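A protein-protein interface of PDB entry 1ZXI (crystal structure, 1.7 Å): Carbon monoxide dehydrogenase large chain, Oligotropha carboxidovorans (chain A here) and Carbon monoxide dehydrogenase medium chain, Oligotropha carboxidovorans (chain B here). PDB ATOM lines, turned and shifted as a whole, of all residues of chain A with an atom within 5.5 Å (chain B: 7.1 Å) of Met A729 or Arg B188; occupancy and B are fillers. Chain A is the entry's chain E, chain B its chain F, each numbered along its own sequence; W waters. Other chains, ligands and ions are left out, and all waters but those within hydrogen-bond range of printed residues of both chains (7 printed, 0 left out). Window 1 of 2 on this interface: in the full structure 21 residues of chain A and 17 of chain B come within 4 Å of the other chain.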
ATOM      1  N   SER A 727      27.363 -26.904 -11.248  1.00  0.00           N
ATOM      2  CA  SER A 727      25.924 -26.658 -11.092  1.00  0.00           C
ATOM      3  C   SER A 727      25.391 -26.686 -12.515  1.00  0.00           C
ATOM      4  O   SER A 727      26.177 -26.623 -13.459  1.00  0.00           O
ATOM      5  CB  SER A 727      25.618 -25.293 -10.461  1.00  0.00           C
ATOM      6  OG  SER A 727      25.707 -24.268 -11.427  1.00  0.00           O
ATOM      7  N   PHE A 728      24.078 -26.796 -12.679  1.00  0.00           N
ATOM      8  CA  PHE A 728      23.509 -26.836 -14.029  1.00  0.00           C
ATOM      9  C   PHE A 728      23.552 -25.484 -14.737  1.00  0.00           C
ATOM     10  O   PHE A 728      23.085 -25.342 -15.864  1.00  0.00           O
ATOM     11  CB  PHE A 728      22.072 -27.399 -14.010  1.00  0.00           C
ATOM     12  CG  PHE A 728      21.998 -28.890 -13.748  1.00  0.00           C
ATOM     13  CD1 PHE A 728      23.156 -29.691 -13.777  1.00  0.00           C
ATOM     14  CD2 PHE A 728      20.774 -29.495 -13.460  1.00  0.00           C
ATOM     15  CE1 PHE A 728      23.083 -31.086 -13.510  1.00  0.00           C
ATOM     16  CE2 PHE A 728      20.684 -30.888 -13.188  1.00  0.00           C
ATOM     17  CZ  PHE A 728      21.838 -31.681 -13.212  1.00  0.00           C
ATOM     18  N   MET A 729      24.112 -24.481 -14.080  1.00  0.00           N
ATOM     19  CA  MET A 729      24.284 -23.184 -14.727  1.00  0.00           C
ATOM     20  C   MET A 729      25.401 -23.341 -15.784  1.00  0.00           C
ATOM     21  O   MET A 729      25.404 -22.656 -16.825  1.00  0.00           O
ATOM     22  CB  MET A 729      24.726 -22.135 -13.702  1.00  0.00           C
ATOM     23  CG  MET A 729      24.594 -20.700 -14.198  1.00  0.00           C
ATOM     24  SD  MET A 729      22.834 -20.162 -14.281  1.00  0.00           S
ATOM     25  CE  MET A 729      22.379 -20.273 -12.576  1.00  0.00           C
ATOM     26  N   ASP A 730      26.346 -24.246 -15.518  1.00  0.00           N
ATOM     27  CA  ASP A 730      27.471 -24.462 -16.430  1.00  0.00           C
ATOM     28  C   ASP A 730      27.710 -25.889 -16.906  1.00  0.00           C
ATOM     29  O   ASP A 730      28.239 -26.087 -17.993  1.00  0.00           O
ATOM     30  CB  ASP A 730      28.774 -23.983 -15.769  1.00  0.00           C
ATOM     31  CG  ASP A 730      28.747 -22.519 -15.424  1.00  0.00           C
ATOM     32  OD1 ASP A 730      28.906 -21.707 -16.359  1.00  0.00           O
ATOM     33  OD2 ASP A 730      28.561 -22.173 -14.225  1.00  0.00           O
ATOM     34  N   PHE A 731      27.336 -26.876 -16.086  1.00  0.00           N
ATOM     35  CA  PHE A 731      27.569 -28.277 -16.406  1.00  0.00           C
ATOM     36  C   PHE A 731      26.682 -28.668 -17.577  1.00  0.00           C
ATOM     37  O   PHE A 731      25.464 -28.699 -17.468  1.00  0.00           O
ATOM     38  CB  PHE A 731      27.278 -29.140 -15.164  1.00  0.00           C
ATOM     39  CG  PHE A 731      27.693 -30.570 -15.309  1.00  0.00           C
ATOM     40  CD1 PHE A 731      29.039 -30.928 -15.209  1.00  0.00           C
ATOM     41  CD2 PHE A 731      26.743 -31.561 -15.550  1.00  0.00           C
ATOM     42  CE1 PHE A 731      29.435 -32.272 -15.347  1.00  0.00           C
ATOM     43  CE2 PHE A 731      27.114 -32.900 -15.690  1.00  0.00           C
ATOM     44  CZ  PHE A 731      28.458 -33.263 -15.589  1.00  0.00           C
ATOM     45  N   PHE A 732      27.319 -29.002 -18.694  1.00  0.00           N
ATOM     46  CA  PHE A 732      26.609 -29.298 -19.920  1.00  0.00           C
ATOM     47  C   PHE A 732      25.789 -30.565 -19.940  1.00  0.00           C
ATOM     48  O   PHE A 732      26.342 -31.649 -20.125  1.00  0.00           O
ATOM     49  CB  PHE A 732      27.617 -29.315 -21.076  1.00  0.00           C
ATOM     50  CG  PHE A 732      26.994 -29.461 -22.443  1.00  0.00           C
ATOM     51  CD1 PHE A 732      26.139 -28.476 -22.959  1.00  0.00           C
ATOM     52  CD2 PHE A 732      27.296 -30.570 -23.230  1.00  0.00           C
ATOM     53  CE1 PHE A 732      25.591 -28.593 -24.245  1.00  0.00           C
ATOM     54  CE2 PHE A 732      26.752 -30.706 -24.530  1.00  0.00           C
ATOM     55  CZ  PHE A 732      25.895 -29.707 -25.035  1.00  0.00           C
ATOM     56  N   GLU A 738      19.737 -29.887 -28.172  1.00  0.00           N
ATOM     57  CA  GLU A 738      21.127 -30.146 -28.525  1.00  0.00           C
ATOM     58  C   GLU A 738      21.450 -31.604 -28.829  1.00  0.00           C
ATOM     59  O   GLU A 738      22.402 -31.887 -29.527  1.00  0.00           O
ATOM     60  CB  GLU A 738      22.072 -29.697 -27.406  1.00  0.00           C
ATOM     61  CG  GLU A 738      22.091 -28.192 -27.117  1.00  0.00           C
ATOM     62  CD  GLU A 738      20.889 -27.741 -26.286  1.00  0.00           C
ATOM     63  OE1 GLU A 738      20.369 -28.538 -25.484  1.00  0.00           O
ATOM     64  OE2 GLU A 738      20.473 -26.583 -26.436  1.00  0.00           O
ATOM     65  N   PRO B  39      15.738 -17.899  -7.377  1.00  0.00           N
ATOM     66  CA  PRO B  39      16.984 -18.666  -7.488  1.00  0.00           C
ATOM     67  C   PRO B  39      18.094 -18.064  -6.601  1.00  0.00           C
ATOM     68  O   PRO B  39      18.824 -18.805  -5.943  1.00  0.00           O
ATOM     69  CB  PRO B  39      17.307 -18.581  -8.980  1.00  0.00           C
ATOM     70  CG  PRO B  39      15.921 -18.644  -9.588  1.00  0.00           C
ATOM     71  CD  PRO B  39      15.140 -17.667  -8.708  1.00  0.00           C
ATOM     72  N   LEU B 186      24.378 -16.331 -29.174  1.00  0.00           N
ATOM     73  CA  LEU B 186      25.290 -17.483 -29.124  1.00  0.00           C
ATOM     74  C   LEU B 186      25.251 -17.939 -27.661  1.00  0.00           C
ATOM     75  O   LEU B 186      25.481 -17.130 -26.769  1.00  0.00           O
ATOM     76  CB  LEU B 186      26.713 -17.071 -29.506  1.00  0.00           C
ATOM     77  CG  LEU B 186      27.773 -18.177 -29.431  1.00  0.00           C
ATOM     78  CD1 LEU B 186      27.435 -19.258 -30.451  1.00  0.00           C
ATOM     79  CD2 LEU B 186      29.155 -17.623 -29.690  1.00  0.00           C
ATOM     80  N   LYS B 187      24.943 -19.215 -27.417  1.00  0.00           N
ATOM     81  CA  LYS B 187      24.865 -19.742 -26.046  1.00  0.00           C
ATOM     82  C   LYS B 187      25.311 -21.205 -26.056  1.00  0.00           C
ATOM     83  O   LYS B 187      25.350 -21.816 -27.119  1.00  0.00           O
ATOM     84  CB  LYS B 187      23.417 -19.648 -25.538  1.00  0.00           C
ATOM     85  CG  LYS B 187      22.454 -20.528 -26.349  1.00  0.00           C
ATOM     86  CD  LYS B 187      20.999 -20.089 -26.198  1.00  0.00           C
ATOM     87  CE  LYS B 187      20.034 -21.046 -26.913  1.00  0.00           C
ATOM     88  NZ  LYS B 187      20.194 -21.066 -28.391  1.00  0.00           N
ATOM     89  N   ARG B 188      25.620 -21.759 -24.881  1.00  0.00           N
ATOM     90  CA  ARG B 188      26.068 -23.154 -24.788  1.00  0.00           C
ATOM     91  C   ARG B 188      24.946 -24.161 -24.964  1.00  0.00           C
ATOM     92  O   ARG B 188      25.186 -25.277 -25.408  1.00  0.00           O
ATOM     93  CB  ARG B 188      26.750 -23.402 -23.432  1.00  0.00           C
ATOM     94  CG  ARG B 188      28.063 -22.633 -23.282  1.00  0.00           C
ATOM     95  CD  ARG B 188      28.629 -22.709 -21.866  1.00  0.00           C
ATOM     96  NE  ARG B 188      27.790 -21.975 -20.920  1.00  0.00           N
ATOM     97  CZ  ARG B 188      28.069 -21.843 -19.628  1.00  0.00           C
ATOM     98  NH1 ARG B 188      29.173 -22.398 -19.122  1.00  0.00           N
ATOM     99  NH2 ARG B 188      27.244 -21.155 -18.847  1.00  0.00           N
ATOM    100  N   LYS B 189      23.730 -23.771 -24.600  1.00  0.00           N
ATOM    101  CA  LYS B 189      22.575 -24.658 -24.706  1.00  0.00           C
ATOM    102  C   LYS B 189      21.317 -23.857 -24.378  1.00  0.00           C
ATOM    103  O   LYS B 189      21.407 -22.725 -23.906  1.00  0.00           O
ATOM    104  CB  LYS B 189      22.713 -25.813 -23.690  1.00  0.00           C
ATOM    105  CG  LYS B 189      22.999 -25.336 -22.255  1.00  0.00           C
ATOM    106  CD  LYS B 189      22.957 -26.447 -21.187  1.00  0.00           C
ATOM    107  CE  LYS B 189      21.519 -26.831 -20.859  1.00  0.00           C
ATOM    108  NZ  LYS B 189      21.399 -27.815 -19.704  1.00  0.00           N
ATOM    109  N   ILE B 190      20.155 -24.461 -24.643  1.00  0.00           N
ATOM    110  CA  ILE B 190      18.859 -23.873 -24.312  1.00  0.00           C
ATOM    111  C   ILE B 190      18.907 -23.424 -22.843  1.00  0.00           C
ATOM    112  O   ILE B 190      19.405 -24.158 -21.969  1.00  0.00           O
ATOM    113  CB  ILE B 190      17.710 -24.947 -24.433  1.00  0.00           C
ATOM    114  CG1 ILE B 190      17.380 -25.202 -25.899  1.00  0.00           C
ATOM    115  CG2 ILE B 190      16.443 -24.503 -23.642  1.00  0.00           C
ATOM    116  CD1 ILE B 190      16.995 -23.947 -26.662  1.00  0.00           C
ATOM    117  N   GLY B 191      18.397 -22.225 -22.578  1.00  0.00           N
ATOM    118  CA  GLY B 191      18.364 -21.725 -21.212  1.00  0.00           C
ATOM    119  C   GLY B 191      19.603 -21.009 -20.711  1.00  0.00           C
ATOM    120  O   GLY B 191      19.581 -20.398 -19.636  1.00  0.00           O
ATOM    121  N   ASP B 192      20.690 -21.074 -21.470  1.00  0.00           N
ATOM    122  CA  ASP B 192      21.945 -20.427 -21.064  1.00  0.00           C
ATOM    123  C   ASP B 192      21.971 -18.939 -21.440  1.00  0.00           C
ATOM    124  O   ASP B 192      21.474 -18.536 -22.495  1.00  0.00           O
ATOM    125  CB  ASP B 192      23.120 -21.179 -21.726  1.00  0.00           C
ATOM    126  CG  ASP B 192      24.511 -20.719 -21.241  1.00  0.00           C
ATOM    127  OD1 ASP B 192      24.677 -20.286 -20.080  1.00  0.00           O
ATOM    128  OD2 ASP B 192      25.458 -20.829 -22.053  1.00  0.00           O
ATOM    129  N   TYR B 193      22.529 -18.114 -20.553  1.00  0.00           N
ATOM    130  CA  TYR B 193      22.675 -16.681 -20.835  1.00  0.00           C
ATOM    131  C   TYR B 193      23.714 -16.599 -21.935  1.00  0.00           C
ATOM    132  O   TYR B 193      24.619 -17.439 -22.030  1.00  0.00           O
ATOM    133  CB  TYR B 193      23.157 -15.936 -19.588  1.00  0.00           C
ATOM    134  CG  TYR B 193      22.148 -16.006 -18.454  1.00  0.00           C
ATOM    135  CD1 TYR B 193      21.070 -15.119 -18.405  1.00  0.00           C
ATOM    136  CD2 TYR B 193      22.250 -16.981 -17.461  1.00  0.00           C
ATOM    137  CE1 TYR B 193      20.128 -15.194 -17.396  1.00  0.00           C
ATOM    138  CE2 TYR B 193      21.302 -17.076 -16.444  1.00  0.00           C
ATOM    139  CZ  TYR B 193      20.250 -16.178 -16.422  1.00  0.00           C
ATOM    140  OH  TYR B 193      19.305 -16.251 -15.436  1.00  0.00           O
ATOM    141  N   ALA B 194      23.592 -15.585 -22.780  1.00  0.00           N
ATOM    142  CA  ALA B 194      24.492 -15.468 -23.917  1.00  0.00           C
ATOM    143  C   ALA B 194      25.988 -15.389 -23.680  1.00  0.00           C
ATOM    144  O   ALA B 194      26.467 -14.739 -22.760  1.00  0.00           O
ATOM    145  CB  ALA B 194      24.087 -14.277 -24.759  1.00  0.00           C
ATOM    146  N   THR B 195      26.708 -16.070 -24.568  1.00  0.00           N
ATOM    147  CA  THR B 195      28.157 -15.983 -24.626  1.00  0.00           C
ATOM    148  C   THR B 195      28.326 -14.552 -25.193  1.00  0.00           C
ATOM    149  O   THR B 195      29.220 -13.797 -24.799  1.00  0.00           O
ATOM    150  CB  THR B 195      28.686 -17.028 -25.616  1.00  0.00           C
ATOM    151  OG1 THR B 195      28.479 -18.337 -25.057  1.00  0.00           O
ATOM    152  CG2 THR B 195      30.177 -16.799 -25.913  1.00  0.00           C
ATOM    153  N   ASP B 259      34.417 -16.618 -18.197  1.00  0.00           N
ATOM    154  CA  ASP B 259      33.770 -17.623 -17.369  1.00  0.00           C
ATOM    155  C   ASP B 259      33.577 -18.900 -18.152  1.00  0.00           C
ATOM    156  O   ASP B 259      34.310 -19.150 -19.120  1.00  0.00           O
ATOM    157  CB  ASP B 259      32.436 -17.092 -16.773  1.00  0.00           C
ATOM    158  CG  ASP B 259      31.408 -16.662 -17.831  1.00  0.00           C
ATOM    159  OD1 ASP B 259      31.340 -17.254 -18.931  1.00  0.00           O
ATOM    160  OD2 ASP B 259      30.628 -15.733 -17.537  1.00  0.00           O
ATOM    161  N   GLY B 260      32.609 -19.714 -17.747  1.00  0.00           N
ATOM    162  CA  GLY B 260      32.377 -20.969 -18.449  1.00  0.00           C
ATOM    163  C   GLY B 260      32.094 -20.855 -19.944  1.00  0.00           C
ATOM    164  O   GLY B 260      32.304 -21.806 -20.696  1.00  0.00           O
ATOM    165  N   ARG B 261      31.626 -19.688 -20.370  1.00  0.00           N
ATOM    166  CA  ARG B 261      31.314 -19.428 -21.768  1.00  0.00           C
ATOM    167  C   ARG B 261      32.570 -19.099 -22.577  1.00  0.00           C
ATOM    168  O   ARG B 261      32.502 -18.931 -23.792  1.00  0.00           O
ATOM    169  CB  ARG B 261      30.303 -18.271 -21.855  1.00  0.00           C
ATOM    170  CG  ARG B 261      28.978 -18.589 -21.139  1.00  0.00           C
ATOM    171  CD  ARG B 261      28.023 -17.390 -21.004  1.00  0.00           C
ATOM    172  NE  ARG B 261      26.887 -17.740 -20.152  1.00  0.00           N
ATOM    173  CZ  ARG B 261      26.923 -17.832 -18.824  1.00  0.00           C
ATOM    174  NH1 ARG B 261      28.041 -17.575 -18.140  1.00  0.00           N
ATOM    175  NH2 ARG B 261      25.848 -18.254 -18.165  1.00  0.00           N
ATOM    176  N   GLY B 262      33.710 -19.000 -21.895  1.00  0.00           N
ATOM    177  CA  GLY B 262      34.951 -18.698 -22.587  1.00  0.00           C
ATOM    178  C   GLY B 262      35.614 -17.415 -22.097  1.00  0.00           C
ATOM    179  O   GLY B 262      35.025 -16.669 -21.301  1.00  0.00           O
HETATM  180  O   HOH W   1      19.600 -19.099 -14.790  1.00  0.00           O
HETATM  181  O   HOH W   2      30.427 -19.799 -15.810  1.00  0.00           O
HETATM  182  O   HOH W   3      20.860 -20.503 -16.979  1.00  0.00           O
HETATM  183  O   HOH W   4      25.080 -23.764 -19.786  1.00  0.00           O
HETATM  184  O   HOH W   5      30.745 -24.737 -19.788  1.00  0.00           O
HETATM  185  O   HOH W   6      23.082 -27.531 -17.458  1.00  0.00           O
HETATM  186  O   HOH W   7      23.675 -20.501 -17.438  1.00  0.00           O
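The guanidinium group (NH1) of Arg B188 lies within salt-bridge range of the side-chain carboxylate (OD1) of Asp A730, 2.9 Å away. OE2 of Glu A738 is in hydrogen-bond range of N of Ile B190, at 2.8 Å. The backbone carbonyl oxygen (O) of Met A729 is in hydrogen-bond range of the guanidinium group (NH2) of Arg B188 (3.1 Å).
The guanidinium group (NE) of Arg B188 is in salt-bridge range of the side-chain carboxylate (OD2) of Asp B192, 2.8 Å away. OG of Ser A727 sits close to N of Met A729 (3.1 Å).
Among the printed residues, merely in contact across the chains: Glu A738 with Lys B189 (3.3 Å) and Phe A732 with Arg B188 (3.5 Å).
Of the printed residues of chain A, Arg B188 touches Met A729 (3.1 Å), Asp A730 (2.9 Å) and Phe A732 (3.5 Å). Of the printed residues of chain B, Phe A732 touches Arg B188. Printed residues of chain B within 4 Å of Asp A730: Arg B188 (2.9 Å). Phe A728 touches none of the printed residues of chain B. The nearest printed residue of chain B that does not touch Met A729 is Tyr B193 (4.1 Å). The nearest residue of chain A that does not touch Arg B188 is Glu A738 (4.6 Å). The nearest printed residue of chain A that does not touch Lys B189 is Phe A732 (4.04 Å).
Of the 7 printed residues of chain A, 4 touch a printed residue of chain B. Hydrophobic or aromatic side chains of chain A that line the printed part of chain B: Phe A732. Of the 15 printed residues of chain B, 3 touch a printed residue of chain A. Hydrophobic or aromatic side chains of chain B within 4 Å of the printed part of chain A: Ile B190. Among the printed residues, 5 pairs touch across the chains. Among the printed residues, Asp or Glu carboxylates within 4 Å of a Lys or Arg side-chain nitrogen of the other chain: Asp A730 with Arg B188.
Water W6 lies within hydrogen-bond range of O of Phe A731 (2.7 Å), O of Phe A728 (2.7 Å) and NZ of Lys B189 (2.8 Å). Water W7 lies within hydrogen-bond range of O of Met A729 (2.8 Å), OD1 of Asp B192 (2.8 Å) and NH2 of Arg B261 (3.2 Å). Water W5 lies within hydrogen-bond range of the guanidinium group (NH1) of Arg B188, the backbone carbonyl oxygen (O) of Asp A730 and the backbone carbonyl oxygen (O) of Gly B260. Water W1 lies within hydrogen-bond range of the side-chain hydroxyl of Tyr B193 (2.9 Å) and the side-chain sulfur of Met A729 (3.4 Å). Water W3 bridges the backbone carbonyl oxygen (O) of Gly B191 (3.0 Å) and the side-chain sulfur (SD) of Met A729 (3.4 Å). Water W4 lies within hydrogen-bond range of the backbone carbonyl oxygen (O) of Met A729 (3.2 Å) and the guanidinium group (NE) of Arg B188 (3.4 Å).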
